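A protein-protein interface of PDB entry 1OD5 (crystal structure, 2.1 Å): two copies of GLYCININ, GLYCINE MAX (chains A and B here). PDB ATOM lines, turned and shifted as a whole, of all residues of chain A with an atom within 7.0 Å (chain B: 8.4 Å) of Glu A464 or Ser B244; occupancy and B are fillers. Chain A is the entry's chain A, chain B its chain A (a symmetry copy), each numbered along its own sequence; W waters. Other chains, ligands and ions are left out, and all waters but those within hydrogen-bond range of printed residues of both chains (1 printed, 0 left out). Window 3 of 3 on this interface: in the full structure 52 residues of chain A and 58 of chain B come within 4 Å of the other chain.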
ATOM      1  N   ILE A 461     -13.951  -6.911  15.426  1.00  0.00           N
ATOM      2  CA  ILE A 461     -14.749  -6.332  14.369  1.00  0.00           C
ATOM      3  C   ILE A 461     -15.485  -7.368  13.551  1.00  0.00           C
ATOM      4  O   ILE A 461     -14.897  -8.410  13.277  1.00  0.00           O
ATOM      5  CB  ILE A 461     -13.761  -5.493  13.541  1.00  0.00           C
ATOM      6  CG1 ILE A 461     -13.119  -4.387  14.372  1.00  0.00           C
ATOM      7  CG2 ILE A 461     -14.509  -4.844  12.427  1.00  0.00           C
ATOM      8  CD1 ILE A 461     -12.012  -3.641  13.598  1.00  0.00           C
ATOM      9  N   PRO A 462     -16.750  -7.180  13.157  1.00  0.00           N
ATOM     10  CA  PRO A 462     -17.482  -8.111  12.305  1.00  0.00           C
ATOM     11  C   PRO A 462     -16.754  -8.501  11.028  1.00  0.00           C
ATOM     12  O   PRO A 462     -16.140  -7.638  10.415  1.00  0.00           O
ATOM     13  CB  PRO A 462     -18.797  -7.414  12.011  1.00  0.00           C
ATOM     14  CG  PRO A 462     -18.990  -6.498  13.195  1.00  0.00           C
ATOM     15  CD  PRO A 462     -17.574  -6.044  13.550  1.00  0.00           C
ATOM     16  N   SER A 463     -16.737  -9.759  10.612  1.00  0.00           N
ATOM     17  CA  SER A 463     -16.093 -10.211   9.404  1.00  0.00           C
ATOM     18  C   SER A 463     -16.475  -9.341   8.219  1.00  0.00           C
ATOM     19  O   SER A 463     -15.585  -8.986   7.455  1.00  0.00           O
ATOM     20  CB  SER A 463     -16.515 -11.610   9.140  1.00  0.00           C
ATOM     21  OG  SER A 463     -15.874 -12.096   7.977  1.00  0.00           O
ATOM     22  N   GLU A 464     -17.736  -8.937   8.034  1.00  0.00           N
ATOM     23  CA  GLU A 464     -18.101  -8.094   6.920  1.00  0.00           C
ATOM     24  C   GLU A 464     -17.581  -6.657   6.984  1.00  0.00           C
ATOM     25  O   GLU A 464     -17.452  -6.117   5.883  1.00  0.00           O
ATOM     26  CB  GLU A 464     -19.610  -8.020   6.756  1.00  0.00           C
ATOM     27  CG  GLU A 464     -20.005  -8.814   5.537  1.00  0.00           C
ATOM     28  CD  GLU A 464     -21.480  -8.775   5.173  1.00  0.00           C
ATOM     29  OE1 GLU A 464     -22.084  -9.852   5.186  1.00  0.00           O
ATOM     30  OE2 GLU A 464     -22.016  -7.710   4.851  1.00  0.00           O
ATOM     31  N   VAL A 465     -17.281  -5.928   8.097  1.00  0.00           N
ATOM     32  CA  VAL A 465     -16.773  -4.564   7.901  1.00  0.00           C
ATOM     33  C   VAL A 465     -15.310  -4.698   7.551  1.00  0.00           C
ATOM     34  O   VAL A 465     -14.784  -3.782   6.949  1.00  0.00           O
ATOM     35  CB  VAL A 465     -16.904  -3.536   9.121  1.00  0.00           C
ATOM     36  CG1 VAL A 465     -18.041  -4.026   9.968  1.00  0.00           C
ATOM     37  CG2 VAL A 465     -15.581  -3.239   9.822  1.00  0.00           C
ATOM     38  N   LEU A 466     -14.649  -5.796   7.903  1.00  0.00           N
ATOM     39  CA  LEU A 466     -13.260  -6.062   7.587  1.00  0.00           C
ATOM     40  C   LEU A 466     -13.203  -6.279   6.073  1.00  0.00           C
ATOM     41  O   LEU A 466     -12.370  -5.708   5.395  1.00  0.00           O
ATOM     42  CB  LEU A 466     -12.856  -7.307   8.358  1.00  0.00           C
ATOM     43  CG  LEU A 466     -11.778  -7.251   9.423  1.00  0.00           C
ATOM     44  CD1 LEU A 466     -11.951  -6.099  10.361  1.00  0.00           C
ATOM     45  CD2 LEU A 466     -11.840  -8.516  10.197  1.00  0.00           C
ATOM     46  N   SER A 467     -14.139  -7.060   5.509  1.00  0.00           N
ATOM     47  CA  SER A 467     -14.228  -7.346   4.094  1.00  0.00           C
ATOM     48  C   SER A 467     -14.349  -6.084   3.294  1.00  0.00           C
ATOM     49  O   SER A 467     -13.563  -5.903   2.385  1.00  0.00           O
ATOM     50  CB  SER A 467     -15.439  -8.164   3.757  1.00  0.00           C
ATOM     51  OG  SER A 467     -14.964  -9.474   3.572  1.00  0.00           O
ATOM     52  N   ASN A 468     -15.317  -5.235   3.634  1.00  0.00           N
ATOM     53  CA  ASN A 468     -15.544  -3.978   2.968  1.00  0.00           C
ATOM     54  C   ASN A 468     -14.459  -2.972   3.227  1.00  0.00           C
ATOM     55  O   ASN A 468     -14.261  -2.058   2.422  1.00  0.00           O
ATOM     56  CB  ASN A 468     -16.809  -3.313   3.423  1.00  0.00           C
ATOM     57  CG  ASN A 468     -18.043  -3.905   2.793  1.00  0.00           C
ATOM     58  OD1 ASN A 468     -18.713  -3.254   1.990  1.00  0.00           O
ATOM     59  ND2 ASN A 468     -18.391  -5.139   3.139  1.00  0.00           N
ATOM     60  N   SER A 469     -13.760  -3.107   4.347  1.00  0.00           N
ATOM     61  CA  SER A 469     -12.730  -2.155   4.652  1.00  0.00           C
ATOM     62  C   SER A 469     -11.474  -2.361   3.834  1.00  0.00           C
ATOM     63  O   SER A 469     -10.895  -1.364   3.396  1.00  0.00           O
ATOM     64  CB  SER A 469     -12.360  -2.206   6.140  1.00  0.00           C
ATOM     65  OG  SER A 469     -13.330  -1.537   6.941  1.00  0.00           O
ATOM     66  N   GLN A 474     -14.441 -13.370   2.217  1.00  0.00           N
ATOM     67  CA  GLN A 474     -14.851 -13.976   3.489  1.00  0.00           C
ATOM     68  C   GLN A 474     -13.840 -14.905   4.154  1.00  0.00           C
ATOM     69  O   GLN A 474     -13.656 -14.872   5.373  1.00  0.00           O
ATOM     70  CB  GLN A 474     -16.146 -14.739   3.278  1.00  0.00           C
ATOM     71  CG  GLN A 474     -16.993 -15.025   4.548  1.00  0.00           C
ATOM     72  CD  GLN A 474     -17.540 -13.797   5.310  1.00  0.00           C
ATOM     73  OE1 GLN A 474     -17.934 -13.935   6.480  1.00  0.00           O
ATOM     74  NE2 GLN A 474     -17.603 -12.579   4.735  1.00  0.00           N
ATOM     75  N   VAL A 477     -10.566 -12.994   5.493  1.00  0.00           N
ATOM     76  CA  VAL A 477     -10.941 -12.335   6.743  1.00  0.00           C
ATOM     77  C   VAL A 477     -10.937 -13.420   7.794  1.00  0.00           C
ATOM     78  O   VAL A 477     -10.364 -13.266   8.874  1.00  0.00           O
ATOM     79  CB  VAL A 477     -12.345 -11.754   6.685  1.00  0.00           C
ATOM     80  CG1 VAL A 477     -12.745 -11.248   8.058  1.00  0.00           C
ATOM     81  CG2 VAL A 477     -12.386 -10.589   5.705  1.00  0.00           C
ATOM     82  N   LYS A 481      -8.671 -13.439  11.479  1.00  0.00           N
ATOM     83  CA  LYS A 481      -9.387 -13.441  12.751  1.00  0.00           C
ATOM     84  C   LYS A 481      -9.066 -14.637  13.621  1.00  0.00           C
ATOM     85  O   LYS A 481      -8.707 -14.493  14.786  1.00  0.00           O
ATOM     86  CB  LYS A 481     -10.869 -13.466  12.520  1.00  0.00           C
ATOM     87  CG  LYS A 481     -11.572 -12.156  12.464  1.00  0.00           C
ATOM     88  CD  LYS A 481     -12.987 -12.521  12.121  1.00  0.00           C
ATOM     89  CE  LYS A 481     -13.863 -11.319  12.374  1.00  0.00           C
ATOM     90  NZ  LYS A 481     -13.970 -11.033  13.788  1.00  0.00           N
ATOM     91  N   LEU B  56     -20.676   3.058   5.544  1.00  0.00           N
ATOM     92  CA  LEU B  56     -19.762   2.490   6.527  1.00  0.00           C
ATOM     93  C   LEU B  56     -18.598   3.450   6.857  1.00  0.00           C
ATOM     94  O   LEU B  56     -17.714   3.568   6.012  1.00  0.00           O
ATOM     95  CB  LEU B  56     -19.141   1.192   5.976  1.00  0.00           C
ATOM     96  CG  LEU B  56     -18.492   0.067   6.822  1.00  0.00           C
ATOM     97  CD1 LEU B  56     -17.374  -0.532   5.987  1.00  0.00           C
ATOM     98  CD2 LEU B  56     -17.857   0.549   8.111  1.00  0.00           C
ATOM     99  N   LEU B  58     -15.193   3.844   8.033  1.00  0.00           N
ATOM    100  CA  LEU B  58     -14.120   2.895   8.317  1.00  0.00           C
ATOM    101  C   LEU B  58     -13.443   3.005   9.663  1.00  0.00           C
ATOM    102  O   LEU B  58     -13.401   4.100  10.203  1.00  0.00           O
ATOM    103  CB  LEU B  58     -13.029   2.983   7.218  1.00  0.00           C
ATOM    104  CG  LEU B  58     -13.420   2.721   5.756  1.00  0.00           C
ATOM    105  CD1 LEU B  58     -12.165   2.720   4.936  1.00  0.00           C
ATOM    106  CD2 LEU B  58     -14.043   1.357   5.537  1.00  0.00           C
ATOM    107  N   LYS B  90     -21.717 -16.487  16.026  1.00  0.00           N
ATOM    108  CA  LYS B  90     -22.635 -17.170  15.146  1.00  0.00           C
ATOM    109  C   LYS B  90     -22.008 -18.488  14.768  1.00  0.00           C
ATOM    110  O   LYS B  90     -20.962 -18.475  14.123  1.00  0.00           O
ATOM    111  CB  LYS B  90     -22.864 -16.369  13.892  1.00  0.00           C
ATOM    112  CG  LYS B  90     -24.092 -16.866  13.191  1.00  0.00           C
ATOM    113  CD  LYS B  90     -24.306 -16.049  11.943  1.00  0.00           C
ATOM    114  CE  LYS B  90     -25.710 -16.246  11.367  1.00  0.00           C
ATOM    115  NZ  LYS B  90     -26.723 -15.471  12.083  1.00  0.00           N
ATOM    116  N   ASP B 108     -18.859 -16.349  12.334  1.00  0.00           N
ATOM    117  CA  ASP B 108     -18.161 -15.198  12.825  1.00  0.00           C
ATOM    118  C   ASP B 108     -18.390 -14.920  14.311  1.00  0.00           C
ATOM    119  O   ASP B 108     -19.281 -15.508  14.927  1.00  0.00           O
ATOM    120  CB  ASP B 108     -18.628 -14.028  11.981  1.00  0.00           C
ATOM    121  CG  ASP B 108     -17.698 -12.838  12.113  1.00  0.00           C
ATOM    122  OD1 ASP B 108     -18.178 -11.737  12.326  1.00  0.00           O
ATOM    123  OD2 ASP B 108     -16.483 -13.011  12.035  1.00  0.00           O
ATOM    124  N   SER B 109     -17.509 -14.089  14.894  1.00  0.00           N
ATOM    125  CA  SER B 109     -17.648 -13.662  16.273  1.00  0.00           C
ATOM    126  C   SER B 109     -17.017 -12.295  16.324  1.00  0.00           C
ATOM    127  O   SER B 109     -16.086 -12.020  15.587  1.00  0.00           O
ATOM    128  CB  SER B 109     -16.929 -14.557  17.250  1.00  0.00           C
ATOM    129  OG  SER B 109     -15.524 -14.449  17.193  1.00  0.00           O
ATOM    130  N   HIS B 110     -17.564 -11.422  17.143  1.00  0.00           N
ATOM    131  CA  HIS B 110     -17.071 -10.065  17.305  1.00  0.00           C
ATOM    132  C   HIS B 110     -17.605  -9.438  18.572  1.00  0.00           C
ATOM    133  O   HIS B 110     -18.488 -10.027  19.206  1.00  0.00           O
ATOM    134  CB  HIS B 110     -17.519  -9.175  16.165  1.00  0.00           C
ATOM    135  CG  HIS B 110     -19.000  -9.100  15.872  1.00  0.00           C
ATOM    136  ND1 HIS B 110     -19.900  -8.324  16.420  1.00  0.00           N
ATOM    137  CD2 HIS B 110     -19.612  -9.796  14.859  1.00  0.00           C
ATOM    138  CE1 HIS B 110     -21.030  -8.494  15.798  1.00  0.00           C
ATOM    139  NE2 HIS B 110     -20.843  -9.382  14.856  1.00  0.00           N
ATOM    140  N   ILE B 113     -22.526  -5.033  19.385  1.00  0.00           N
ATOM    141  CA  ILE B 113     -22.942  -4.041  18.396  1.00  0.00           C
ATOM    142  C   ILE B 113     -23.921  -3.160  19.149  1.00  0.00           C
ATOM    143  O   ILE B 113     -24.803  -3.692  19.828  1.00  0.00           O
ATOM    144  CB  ILE B 113     -23.690  -4.691  17.189  1.00  0.00           C
ATOM    145  CG1 ILE B 113     -22.738  -5.591  16.461  1.00  0.00           C
ATOM    146  CG2 ILE B 113     -24.248  -3.649  16.221  1.00  0.00           C
ATOM    147  CD1 ILE B 113     -21.584  -4.847  15.794  1.00  0.00           C
ATOM    148  N   TRP B 131     -16.287   2.077  14.332  1.00  0.00           N
ATOM    149  CA  TRP B 131     -16.806   2.131  12.980  1.00  0.00           C
ATOM    150  C   TRP B 131     -18.304   2.328  13.129  1.00  0.00           C
ATOM    151  O   TRP B 131     -18.885   1.965  14.150  1.00  0.00           O
ATOM    152  CB  TRP B 131     -16.506   0.815  12.215  1.00  0.00           C
ATOM    153  CG  TRP B 131     -17.051  -0.476  12.815  1.00  0.00           C
ATOM    154  CD1 TRP B 131     -16.265  -1.275  13.612  1.00  0.00           C
ATOM    155  CD2 TRP B 131     -18.332  -0.942  12.689  1.00  0.00           C
ATOM    156  NE1 TRP B 131     -17.057  -2.244  14.015  1.00  0.00           N
ATOM    157  CE2 TRP B 131     -18.293  -2.085  13.495  1.00  0.00           C
ATOM    158  CE3 TRP B 131     -19.509  -0.569  12.042  1.00  0.00           C
ATOM    159  CZ2 TRP B 131     -19.438  -2.869  13.648  1.00  0.00           C
ATOM    160  CZ3 TRP B 131     -20.653  -1.353  12.198  1.00  0.00           C
ATOM    161  CH2 TRP B 131     -20.617  -2.493  12.999  1.00  0.00           C
ATOM    162  N   TYR B 133     -22.251   2.425  10.802  1.00  0.00           N
ATOM    163  CA  TYR B 133     -22.847   2.007   9.555  1.00  0.00           C
ATOM    164  C   TYR B 133     -24.270   2.478   9.577  1.00  0.00           C
ATOM    165  O   TYR B 133     -24.933   2.378  10.605  1.00  0.00           O
ATOM    166  CB  TYR B 133     -22.771   0.516   9.457  1.00  0.00           C
ATOM    167  CG  TYR B 133     -23.619  -0.004   8.333  1.00  0.00           C
ATOM    168  CD1 TYR B 133     -23.250   0.199   6.997  1.00  0.00           C
ATOM    169  CD2 TYR B 133     -24.773  -0.697   8.646  1.00  0.00           C
ATOM    170  CE1 TYR B 133     -24.039  -0.300   5.967  1.00  0.00           C
ATOM    171  CE2 TYR B 133     -25.566  -1.200   7.621  1.00  0.00           C
ATOM    172  CZ  TYR B 133     -25.192  -1.002   6.298  1.00  0.00           C
ATOM    173  OH  TYR B 133     -25.965  -1.551   5.305  1.00  0.00           O
ATOM    174  N   VAL B 237     -17.278   4.578   3.069  1.00  0.00           N
ATOM    175  CA  VAL B 237     -17.616   3.823   1.873  1.00  0.00           C
ATOM    176  C   VAL B 237     -19.069   3.332   1.814  1.00  0.00           C
ATOM    177  O   VAL B 237     -19.800   3.325   2.803  1.00  0.00           O
ATOM    178  CB  VAL B 237     -16.645   2.618   1.766  1.00  0.00           C
ATOM    179  CG1 VAL B 237     -15.223   3.125   1.961  1.00  0.00           C
ATOM    180  CG2 VAL B 237     -16.978   1.540   2.802  1.00  0.00           C
ATOM    181  N   VAL B 239     -21.700   0.285   1.135  1.00  0.00           N
ATOM    182  CA  VAL B 239     -21.705  -1.156   1.225  1.00  0.00           C
ATOM    183  C   VAL B 239     -22.877  -1.546   0.352  1.00  0.00           C
ATOM    184  O   VAL B 239     -24.046  -1.328   0.688  1.00  0.00           O
ATOM    185  CB  VAL B 239     -21.921  -1.624   2.677  1.00  0.00           C
ATOM    186  CG1 VAL B 239     -21.811  -3.134   2.703  1.00  0.00           C
ATOM    187  CG2 VAL B 239     -20.863  -1.063   3.616  1.00  0.00           C
ATOM    188  N   GLU B 240     -22.513  -2.076  -0.822  1.00  0.00           N
ATOM    189  CA  GLU B 240     -23.503  -2.514  -1.794  1.00  0.00           C
ATOM    190  C   GLU B 240     -23.997  -3.879  -1.339  1.00  0.00           C
ATOM    191  O   GLU B 240     -23.242  -4.812  -1.048  1.00  0.00           O
ATOM    192  CB  GLU B 240     -22.878  -2.612  -3.204  1.00  0.00           C
ATOM    193  CG  GLU B 240     -23.964  -2.737  -4.306  1.00  0.00           C
ATOM    194  CD  GLU B 240     -23.534  -2.862  -5.786  1.00  0.00           C
ATOM    195  OE1 GLU B 240     -24.391  -3.270  -6.578  1.00  0.00           O
ATOM    196  OE2 GLU B 240     -22.385  -2.553  -6.157  1.00  0.00           O
ATOM    197  N   GLY B 241     -25.329  -3.942  -1.284  1.00  0.00           N
ATOM    198  CA  GLY B 241     -26.047  -5.148  -0.849  1.00  0.00           C
ATOM    199  C   GLY B 241     -26.513  -4.901   0.579  1.00  0.00           C
ATOM    200  O   GLY B 241     -27.697  -4.849   0.921  1.00  0.00           O
ATOM    201  N   GLY B 242     -25.507  -4.620   1.393  1.00  0.00           N
ATOM    202  CA  GLY B 242     -25.731  -4.343   2.779  1.00  0.00           C
ATOM    203  C   GLY B 242     -24.658  -5.042   3.550  1.00  0.00           C
ATOM    204  O   GLY B 242     -23.879  -5.885   3.098  1.00  0.00           O
ATOM    205  N   LEU B 243     -24.612  -4.514   4.754  1.00  0.00           N
ATOM    206  CA  LEU B 243     -23.689  -5.021   5.731  1.00  0.00           C
ATOM    207  C   LEU B 243     -24.552  -5.887   6.631  1.00  0.00           C
ATOM    208  O   LEU B 243     -25.715  -5.582   6.901  1.00  0.00           O
ATOM    209  CB  LEU B 243     -23.120  -3.915   6.551  1.00  0.00           C
ATOM    210  CG  LEU B 243     -21.985  -4.323   7.439  1.00  0.00           C
ATOM    211  CD1 LEU B 243     -20.760  -4.595   6.583  1.00  0.00           C
ATOM    212  CD2 LEU B 243     -21.740  -3.230   8.462  1.00  0.00           C
ATOM    213  N   SER B 244     -24.011  -7.021   7.034  1.00  0.00           N
ATOM    214  CA  SER B 244     -24.731  -7.877   7.933  1.00  0.00           C
ATOM    215  C   SER B 244     -23.685  -8.417   8.880  1.00  0.00           C
ATOM    216  O   SER B 244     -22.626  -8.935   8.517  1.00  0.00           O
ATOM    217  CB  SER B 244     -25.426  -9.001   7.192  1.00  0.00           C
ATOM    218  OG  SER B 244     -24.491  -9.784   6.490  1.00  0.00           O
ATOM    219  N   VAL B 245     -24.001  -8.057  10.129  1.00  0.00           N
ATOM    220  CA  VAL B 245     -23.219  -8.419  11.313  1.00  0.00           C
ATOM    221  C   VAL B 245     -24.142  -9.186  12.282  1.00  0.00           C
ATOM    222  O   VAL B 245     -25.348  -9.277  12.017  1.00  0.00           O
ATOM    223  CB  VAL B 245     -22.670  -7.149  11.996  1.00  0.00           C
ATOM    224  CG1 VAL B 245     -21.923  -6.297  10.970  1.00  0.00           C
ATOM    225  CG2 VAL B 245     -23.802  -6.326  12.589  1.00  0.00           C
ATOM    226  N   ILE B 246     -23.623  -9.783  13.378  1.00  0.00           N
ATOM    227  CA  ILE B 246     -24.440 -10.509  14.365  1.00  0.00           C
ATOM    228  C   ILE B 246     -25.087  -9.506  15.316  1.00  0.00           C
ATOM    229  O   ILE B 246     -24.389  -8.757  15.983  1.00  0.00           O
ATOM    230  CB  ILE B 246     -23.552 -11.476  15.156  1.00  0.00           C
ATOM    231  CG1 ILE B 246     -22.815 -12.387  14.200  1.00  0.00           C
ATOM    232  CG2 ILE B 246     -24.405 -12.321  16.096  1.00  0.00           C
ATOM    233  CD1 ILE B 246     -21.557 -12.955  14.876  1.00  0.00           C
ATOM    234  N   SER B 247     -26.419  -9.441  15.342  1.00  0.00           N
ATOM    235  CA  SER B 247     -27.173  -8.540  16.205  1.00  0.00           C
ATOM    236  C   SER B 247     -28.577  -9.107  16.436  1.00  0.00           C
ATOM    237  O   SER B 247     -29.149  -9.708  15.514  1.00  0.00           O
ATOM    238  CB  SER B 247     -27.301  -7.157  15.560  1.00  0.00           C
ATOM    239  OG  SER B 247     -28.038  -6.229  16.337  1.00  0.00           O
ATOM    240  N   TRP B 250     -32.007  -6.870  13.948  1.00  0.00           N
ATOM    241  CA  TRP B 250     -31.630  -6.641  12.557  1.00  0.00           C
ATOM    242  C   TRP B 250     -32.089  -7.772  11.644  1.00  0.00           C
ATOM    243  O   TRP B 250     -32.519  -7.460  10.526  1.00  0.00           O
ATOM    244  CB  TRP B 250     -30.119  -6.509  12.373  1.00  0.00           C
ATOM    245  CG  TRP B 250     -29.762  -5.545  11.230  1.00  0.00           C
ATOM    246  CD1 TRP B 250     -30.701  -4.812  10.502  1.00  0.00           C
ATOM    247  CD2 TRP B 250     -28.481  -5.291  10.813  1.00  0.00           C
ATOM    248  NE1 TRP B 250     -30.008  -4.103   9.636  1.00  0.00           N
ATOM    249  CE2 TRP B 250     -28.689  -4.354   9.786  1.00  0.00           C
ATOM    250  CE3 TRP B 250     -27.202  -5.706  11.162  1.00  0.00           C
ATOM    251  CZ2 TRP B 250     -27.594  -3.825   9.096  1.00  0.00           C
ATOM    252  CZ3 TRP B 250     -26.118  -5.167  10.465  1.00  0.00           C
ATOM    253  CH2 TRP B 250     -26.305  -4.238   9.447  1.00  0.00           C
HETATM  254  O   HOH W   1     -22.774 -11.971   7.600  1.00  0.00           O
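NZ of Lys A481 lies within hydrogen-bond range of O of Ser B109, at 2.9 Å. O of Gly B242 lies close to OE2 of Glu A464, at 3.1 Å. NZ of Lys A481 lies within salt-bridge range of OD2 of Asp B108 (3.6 Å). The backbone NH (N) of Ser A463 lies within hydrogen-bond range of the side-chain carboxylate (OD1) of Asp B108. OE1 of Glu A464 is in hydrogen-bond range of OG of Ser B244 (2.7 Å).
Of the 12 printed residues of chain A, 7 touch a printed residue of chain B. Hydrophobic or aromatic side chains of chain A that line the printed part of chain B: Ile A461 and Pro A462. Along chain A the printed residues that touch a printed residue of chain B span positions 461 to 481. Printed residues of chain B that touch a printed residue of chain A: Leu B56, Leu B58, Asp B108, Ser B109, His B110, Trp B131, Val B239, Gly B242, Leu B243, Ser B244 and Val B245. Hydrophobic or aromatic side chains of chain B within 4 Å of the printed part of chain A: Leu B56, Leu B58, His B110, Trp B131, Val B239, Leu B243 and Val B245. Among the printed residues, 15 pairs touch across the chains. Among the printed residues, Asp or Glu carboxylates within 4 Å of a Lys or Arg side-chain nitrogen of the other chain: Lys A481 with Asp B108 (3.6 Å).
Water W1 lies within hydrogen-bond range of the side-chain hydroxyl of Ser B244 and the side-chain carboxylate of Glu A464.
CB of His B110 touches C of Ile A461, at 3.8 Å. NE1 of Trp B131 touches CG2 of Ile A461, 3.97 Å away. Pro A462 touches Asp B108. CB of His B110 touches N of Pro A462, at 3.7 Å. Pro A462 touches Trp B131. Val B245 touches Pro A462. Glu A464 touches Leu B243 (OE2 to CA, 3.3 Å). Leu B56 touches Asn A468. CG1 of Val B239 touches OD1 of Asn A468, 3.2 Å away. Ser A469 touches Leu B58 (OG to CD2, 3.3 Å).
Of chain B, only Gly B242, Leu B243 and Ser B244 come within 4 Å of Glu A464. Of chain B, only Asp B108 (3.0 Å) comes within 4 Å of Ser A463. Of the printed residues of chain A, Trp B131 touches Ile A461 and Pro A462. Of the printed residues of chain B, Pro A462 touches Asp B108 (3.7 Å), His B110 (3.7 Å), Trp B131 (3.7 Å) and Val B245 (3.5 Å). Printed residues of chain A within 4 Å of Gly B242: Glu A464 (3.1 Å). Tyr B133 touches none of the printed residues of chain A. Val A477 touches none of the printed residues of chain B. The nearest residue of chain A that does not touch Ser B244 is Pro A462 (5.4 Å).
N of Lys B90 lies within hydrogen-bond range of O of Asp B108. The side-chain hydroxyl (OH) of Tyr B133 lies within hydrogen-bond range of the backbone NH (N) of Leu B243, at 3.3 Å. ND2 of Asn A468 lies within hydrogen-bond range of O of Glu A464 (3.1 Å). The backbone NH of Leu B56 is in hydrogen-bond range of the backbone carbonyl oxygen of Val B237 (2.9 Å). O of Ile A461 lies within hydrogen-bond range of NZ of Lys A481. A ring nitrogen (NE2) of His B110 lies within hydrogen-bond range of the backbone NH of Ile B246.
No position is printed for both chains. Of the 15 pairs that touch across the chains among the printed residues, none has its exchanged pair printed and touching as well.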
